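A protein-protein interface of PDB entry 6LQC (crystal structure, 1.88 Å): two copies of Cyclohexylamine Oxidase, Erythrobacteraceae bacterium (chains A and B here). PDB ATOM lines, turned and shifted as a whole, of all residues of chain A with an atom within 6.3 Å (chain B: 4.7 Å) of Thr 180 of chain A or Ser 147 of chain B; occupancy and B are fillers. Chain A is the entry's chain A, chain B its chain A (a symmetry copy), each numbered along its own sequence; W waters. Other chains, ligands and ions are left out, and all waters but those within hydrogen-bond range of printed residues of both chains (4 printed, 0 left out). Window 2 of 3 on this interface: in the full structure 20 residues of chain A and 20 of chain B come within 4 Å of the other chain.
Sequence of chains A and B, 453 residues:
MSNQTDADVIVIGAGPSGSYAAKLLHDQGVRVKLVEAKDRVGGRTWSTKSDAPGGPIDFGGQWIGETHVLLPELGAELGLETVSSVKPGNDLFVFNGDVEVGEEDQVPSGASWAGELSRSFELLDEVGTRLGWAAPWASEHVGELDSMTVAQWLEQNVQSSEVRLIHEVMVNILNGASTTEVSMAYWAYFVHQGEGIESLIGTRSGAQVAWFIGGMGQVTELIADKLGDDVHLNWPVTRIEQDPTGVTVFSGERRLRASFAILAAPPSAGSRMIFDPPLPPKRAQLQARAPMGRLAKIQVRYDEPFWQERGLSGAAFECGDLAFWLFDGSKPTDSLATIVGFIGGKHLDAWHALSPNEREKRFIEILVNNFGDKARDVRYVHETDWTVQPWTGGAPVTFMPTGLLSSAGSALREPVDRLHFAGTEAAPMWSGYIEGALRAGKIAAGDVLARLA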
ATOM      1  N   THR A 149      15.587 -10.190  20.918  1.00  0.00           N
ATOM      2  CA  THR A 149      15.342  -9.087  21.868  1.00  0.00           C
ATOM      3  C   THR A 149      16.190  -9.284  23.110  1.00  0.00           C
ATOM      4  O   THR A 149      16.690 -10.444  23.391  1.00  0.00           O
ATOM      5  CB  THR A 149      13.875  -9.038  22.243  1.00  0.00           C
ATOM      6  OG1 THR A 149      13.567 -10.176  23.069  1.00  0.00           O
ATOM      7  CG2 THR A 149      13.000  -9.037  21.014  1.00  0.00           C
ATOM      8  N   VAL A 150      16.284  -8.237  23.896  1.00  0.00           N
ATOM      9  CA  VAL A 150      16.995  -8.311  25.197  1.00  0.00           C
ATOM     10  C   VAL A 150      16.223  -9.328  26.069  1.00  0.00           C
ATOM     11  O   VAL A 150      16.868 -10.149  26.777  1.00  0.00           O
ATOM     12  CB  VAL A 150      17.107  -6.946  25.862  1.00  0.00           C
ATOM     13  CG1 VAL A 150      17.717  -7.076  27.230  1.00  0.00           C
ATOM     14  CG2 VAL A 150      17.918  -5.953  25.055  1.00  0.00           C
ATOM     15  N   ALA A 151      14.897  -9.320  26.003  1.00  0.00           N
ATOM     16  CA  ALA A 151      14.089 -10.215  26.846  1.00  0.00           C
ATOM     17  C   ALA A 151      14.491 -11.663  26.529  1.00  0.00           C
ATOM     18  O   ALA A 151      14.580 -12.449  27.494  1.00  0.00           O
ATOM     19  CB  ALA A 151      12.615 -10.018  26.672  1.00  0.00           C
ATOM     20  N   GLN A 152      14.633 -12.009  25.246  1.00  0.00           N
ATOM     21  CA  GLN A 152      14.975 -13.393  24.839  1.00  0.00           C
ATOM     22  C   GLN A 152      16.385 -13.724  25.347  1.00  0.00           C
ATOM     23  O   GLN A 152      16.628 -14.876  25.788  1.00  0.00           O
ATOM     24  CB  GLN A 152      14.822 -13.587  23.343  1.00  0.00           C
ATOM     25  CG  GLN A 152      13.379 -13.501  22.898  1.00  0.00           C
ATOM     26  CD  GLN A 152      13.211 -13.199  21.429  1.00  0.00           C
ATOM     27  OE1 GLN A 152      14.099 -12.657  20.760  1.00  0.00           O
ATOM     28  NE2 GLN A 152      12.095 -13.659  20.890  1.00  0.00           N
ATOM     29  N   ALA A 177      12.707   1.712  26.852  1.00  0.00           N
ATOM     30  CA  ALA A 177      11.942   0.723  26.080  1.00  0.00           C
ATOM     31  C   ALA A 177      12.002  -0.642  26.796  1.00  0.00           C
ATOM     32  O   ALA A 177      12.890  -0.869  27.619  1.00  0.00           O
ATOM     33  CB  ALA A 177      12.462   0.632  24.669  1.00  0.00           C
ATOM     34  N   SER A 178      11.045  -1.467  26.486  1.00  0.00           N
ATOM     35  CA  SER A 178      10.873  -2.808  27.086  1.00  0.00           C
ATOM     36  C   SER A 178      11.958  -3.730  26.547  1.00  0.00           C
ATOM     37  O   SER A 178      12.413  -3.592  25.402  1.00  0.00           O
ATOM     38  CB  SER A 178       9.512  -3.331  26.790  1.00  0.00           C
ATOM     39  OG  SER A 178       9.380  -4.641  27.309  1.00  0.00           O
ATOM     40  N   THR A 179      12.362  -4.702  27.349  1.00  0.00           N
ATOM     41  CA  THR A 179      13.306  -5.753  26.915  1.00  0.00           C
ATOM     42  C   THR A 179      12.709  -6.550  25.762  1.00  0.00           C
ATOM     43  O   THR A 179      13.476  -7.117  25.010  1.00  0.00           O
ATOM     44  CB  THR A 179      13.631  -6.681  28.085  1.00  0.00           C
ATOM     45  OG1 THR A 179      12.408  -7.204  28.592  1.00  0.00           O
ATOM     46  CG2 THR A 179      14.414  -5.983  29.153  1.00  0.00           C
ATOM     47  N   THR A 180      11.388  -6.572  25.601  1.00  0.00           N
ATOM     48  CA  THR A 180      10.735  -7.242  24.448  1.00  0.00           C
ATOM     49  C   THR A 180      10.845  -6.377  23.180  1.00  0.00           C
ATOM     50  O   THR A 180      10.539  -6.925  22.086  1.00  0.00           O
ATOM     51  CB  THR A 180       9.283  -7.609  24.747  1.00  0.00           C
ATOM     52  OG1 THR A 180       8.593  -6.372  24.958  1.00  0.00           O
ATOM     53  CG2 THR A 180       9.123  -8.513  25.956  1.00  0.00           C
ATOM     54  N   GLU A 181      11.165  -5.073  23.296  1.00  0.00           N
ATOM     55  CA  GLU A 181      11.140  -4.143  22.120  1.00  0.00           C
ATOM     56  C   GLU A 181      12.551  -3.865  21.586  1.00  0.00           C
ATOM     57  O   GLU A 181      12.678  -3.522  20.418  1.00  0.00           O
ATOM     58  CB  GLU A 181      10.479  -2.823  22.532  1.00  0.00           C
ATOM     59  CG  GLU A 181       9.013  -2.952  22.933  1.00  0.00           C
ATOM     60  CD  GLU A 181       8.425  -1.798  23.774  1.00  0.00           C
ATOM     61  OE1 GLU A 181       9.178  -0.924  24.218  1.00  0.00           O
ATOM     62  OE2 GLU A 181       7.202  -1.802  24.012  1.00  0.00           O
ATOM     63  N   VAL A 182      13.587  -3.959  22.425  1.00  0.00           N
ATOM     64  CA  VAL A 182      14.952  -3.561  22.047  1.00  0.00           C
ATOM     65  C   VAL A 182      15.691  -4.764  21.508  1.00  0.00           C
ATOM     66  O   VAL A 182      15.612  -5.866  22.116  1.00  0.00           O
ATOM     67  CB  VAL A 182      15.686  -2.947  23.234  1.00  0.00           C
ATOM     68  CG1 VAL A 182      17.053  -2.467  22.828  1.00  0.00           C
ATOM     69  CG2 VAL A 182      14.913  -1.801  23.853  1.00  0.00           C
ATOM     70  N   GLY B 143       0.520 -11.239  24.049  1.00  0.00           N
ATOM     71  CA  GLY B 143       1.756 -10.753  24.685  1.00  0.00           C
ATOM     72  C   GLY B 143       2.937 -11.606  24.301  1.00  0.00           C
ATOM     73  O   GLY B 143       4.009 -11.061  23.882  1.00  0.00           O
ATOM     74  N   GLU B 144       2.745 -12.914  24.354  1.00  0.00           N
ATOM     75  CA  GLU B 144       3.830 -13.869  24.074  1.00  0.00           C
ATOM     76  C   GLU B 144       4.133 -13.872  22.575  1.00  0.00           C
ATOM     77  O   GLU B 144       5.327 -13.832  22.240  1.00  0.00           O
ATOM     78  CB  GLU B 144       3.435 -15.252  24.594  1.00  0.00           C
ATOM     79  CG  GLU B 144       4.544 -16.270  24.455  1.00  0.00           C
ATOM     80  CD  GLU B 144       4.322 -17.545  25.247  1.00  0.00           C
ATOM     81  OE1 GLU B 144       3.658 -17.478  26.295  1.00  0.00           O
ATOM     82  OE2 GLU B 144       4.825 -18.588  24.812  1.00  0.00           O
ATOM     83  N   LEU B 145       3.124 -13.935  21.697  1.00  0.00           N
ATOM     84  CA  LEU B 145       3.361 -13.932  20.232  1.00  0.00           C
ATOM     85  C   LEU B 145       4.016 -12.601  19.815  1.00  0.00           C
ATOM     86  O   LEU B 145       4.781 -12.597  18.836  1.00  0.00           O
ATOM     87  CB  LEU B 145       2.050 -14.093  19.456  1.00  0.00           C
ATOM     88  CG  LEU B 145       1.511 -15.502  19.325  1.00  0.00           C
ATOM     89  CD1 LEU B 145       0.068 -15.454  18.866  1.00  0.00           C
ATOM     90  CD2 LEU B 145       2.385 -16.308  18.387  1.00  0.00           C
ATOM     91  N   ASP B 146       3.630 -11.511  20.471  1.00  0.00           N
ATOM     92  CA  ASP B 146       4.070 -10.140  20.105  1.00  0.00           C
ATOM     93  C   ASP B 146       5.499  -9.940  20.637  1.00  0.00           C
ATOM     94  O   ASP B 146       6.109  -8.903  20.303  1.00  0.00           O
ATOM     95  CB  ASP B 146       3.165  -9.048  20.700  1.00  0.00           C
ATOM     96  CG  ASP B 146       3.271  -7.708  19.952  1.00  0.00           C
ATOM     97  OD1 ASP B 146       3.549  -7.740  18.725  1.00  0.00           O
ATOM     98  OD2 ASP B 146       3.086  -6.686  20.606  1.00  0.00           O
ATOM     99  N   SER B 147       6.047 -10.895  21.395  1.00  0.00           N
ATOM    100  CA  SER B 147       7.432 -10.789  21.906  1.00  0.00           C
ATOM    101  C   SER B 147       8.406 -11.561  21.033  1.00  0.00           C
ATOM    102  O   SER B 147       9.586 -11.592  21.386  1.00  0.00           O
ATOM    103  CB  SER B 147       7.539 -11.211  23.360  1.00  0.00           C
ATOM    104  OG  SER B 147       6.643 -10.425  24.106  1.00  0.00           O
ATOM    105  N   MET B 148       7.960 -12.084  19.900  1.00  0.00           N
ATOM    106  CA  MET B 148       8.845 -12.889  19.040  1.00  0.00           C
ATOM    107  C   MET B 148       8.640 -12.456  17.602  1.00  0.00           C
ATOM    108  O   MET B 148       7.577 -11.891  17.295  1.00  0.00           O
ATOM    109  CB  MET B 148       8.555 -14.393  19.179  1.00  0.00           C
ATOM    110  CG  MET B 148       7.332 -14.841  18.412  1.00  0.00           C
ATOM    111  SD  MET B 148       6.842 -16.548  18.880  1.00  0.00           S
ATOM    112  CE  MET B 148       8.103 -17.498  18.070  1.00  0.00           C
ATOM    113  N   THR B 149       9.640 -12.707  16.782  1.00  0.00           N
ATOM    114  CA  THR B 149       9.594 -12.337  15.354  1.00  0.00           C
ATOM    115  C   THR B 149       9.011 -13.482  14.547  1.00  0.00           C
ATOM    116  O   THR B 149       8.977 -14.681  15.032  1.00  0.00           O
ATOM    117  CB  THR B 149      10.985 -12.006  14.856  1.00  0.00           C
ATOM    118  OG1 THR B 149      11.758 -13.220  14.792  1.00  0.00           O
ATOM    119  CG2 THR B 149      11.663 -11.007  15.760  1.00  0.00           C
ATOM    120  N   GLN B 152      11.642 -16.193  14.176  1.00  0.00           N
ATOM    121  CA  GLN B 152      11.755 -17.115  15.331  1.00  0.00           C
ATOM    122  C   GLN B 152      10.613 -18.138  15.262  1.00  0.00           C
ATOM    123  O   GLN B 152      10.833 -19.333  15.583  1.00  0.00           O
ATOM    124  CB  GLN B 152      11.797 -16.358  16.645  1.00  0.00           C
ATOM    125  CG  GLN B 152      13.063 -15.544  16.797  1.00  0.00           C
ATOM    126  CD  GLN B 152      12.950 -14.426  17.805  1.00  0.00           C
ATOM    127  OE1 GLN B 152      11.861 -13.949  18.143  1.00  0.00           O
ATOM    128  NE2 GLN B 152      14.088 -14.079  18.381  1.00  0.00           N
ATOM    129  N   THR B 402       8.315  -6.112  17.363  1.00  0.00           N
ATOM    130  CA  THR B 402       7.910  -6.742  18.634  1.00  0.00           C
ATOM    131  C   THR B 402       7.395  -5.687  19.613  1.00  0.00           C
ATOM    132  O   THR B 402       8.053  -4.610  19.775  1.00  0.00           O
ATOM    133  CB  THR B 402       9.049  -7.543  19.261  1.00  0.00           C
ATOM    134  OG1 THR B 402      10.252  -6.792  19.485  1.00  0.00           O
ATOM    135  CG2 THR B 402       9.377  -8.701  18.354  1.00  0.00           C
ATOM    136  N   GLY B 403       6.305  -6.039  20.308  1.00  0.00           N
ATOM    137  CA  GLY B 403       5.842  -5.329  21.520  1.00  0.00           C
ATOM    138  C   GLY B 403       4.830  -4.239  21.208  1.00  0.00           C
ATOM    139  O   GLY B 403       4.142  -3.784  22.151  1.00  0.00           O
HETATM  140  O   HOH W   1      10.123  -2.831  19.095  1.00  0.00           O
HETATM  141  O   HOH W   2      10.973 -10.723  23.539  1.00  0.00           O
HETATM  142  O   HOH W   3      12.530  -5.618  18.464  1.00  0.00           O
HETATM  143  O   HOH W   4       5.578  -3.651  24.876  1.00  0.00           O
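The backbone carbonyl oxygen of Thr 180 of chain A sits at hydrogen-bond distance from the side-chain hydroxyl of Thr 402 of chain B (2.6 Å).
NE2 of Gln 152 of chain A lies within hydrogen-bond range of O of Ser 147 of chain B (3.3 Å).
The side-chain amide oxygen of Gln 152 of chain A is in hydrogen-bond range of the side-chain amide nitrogen of Gln 152 of chain B (2.8 Å).
The backbone NH (N) of Ser 178 of chain A is in hydrogen-bond range of the side-chain carboxylate (OE1) of Glu 181 of chain A, at 3.0 Å.
The backbone carbonyl oxygen (O) of Gly 143 of chain B is in hydrogen-bond range of the side-chain hydroxyl (OG) of Ser 147 of chain B, 2.7 Å away.
OG1 of Thr 149 of chain A lies close to N of Ala 151 of chain A, at 3.3 Å.
The backbone NH (N) of Thr 149 of chain B sits at hydrogen-bond distance from the side-chain amide oxygen (OE1) of Gln 152 of chain B.
OG of Ser 178 of chain A sits at hydrogen-bond distance from OG1 of Thr 180 of chain A, 3.0 Å away.
The backbone NH (N) of Thr 149 of chain A is in hydrogen-bond range of the side-chain amide oxygen (OE1) of Gln 152 of chain A, 2.9 Å away.
Among the printed residues, pairs that only touch across the chains: Thr 180 of chain A with Ser 147 of chain B (3.6 Å), Glu 181 of chain A with Thr 402 of chain B (3.7 Å), Gln 152 of chain A with Met 148 of chain B (3.8 Å) and Thr 149 of chain A with Thr 402 of chain B (3.9 Å).
Printed residues of chain B within 4 Å of Thr 149 of chain A: Thr 402 (3.9 Å).
Ser 178 of chain A touches none of the printed residues of chain B.
Of chain B, only Ser 147 (3.6 Å) and Thr 402 (2.6 Å) come within 4 Å of Thr 180 of chain A.
Of the printed residues of chain A, Thr 402 of chain B touches Thr 149, Thr 180 and Glu 181.
The nearest residue of chain B that does not touch Thr 180 of chain A is Gly 403 of chain B (4.5 Å).
Of the 10 printed residues of chain A, 4 touch a printed residue of chain B.
Along chain A the printed residues that touch a printed residue of chain B span positions 149 to 181.
Among the printed residues, 7 pairs touch across the chains.
Gln 152 of chain A touches its own counterpart, Gln 152 of chain B.
Positions printed for both chains: 149 and 152.
Of the 7 pairs that touch across the chains among the printed residues, 1 has its exchanged pair printed and touching as well.
Water W4 lies within hydrogen-bond range of OE2 of Glu 181 of chain A and O of Gly 403 of chain B.
Water W2 lies within hydrogen-bond range of OG1 of Thr 149 of chain A (2.7 Å) and O of Ser 147 of chain B (2.7 Å).
Water W3 bridges OG1 of Thr 402 of chain B and O of Glu 181 of chain A.
Water W1 bridges O of Thr 402 of chain B (2.8 Å) and O of Glu 181 of chain A (3.0 Å).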
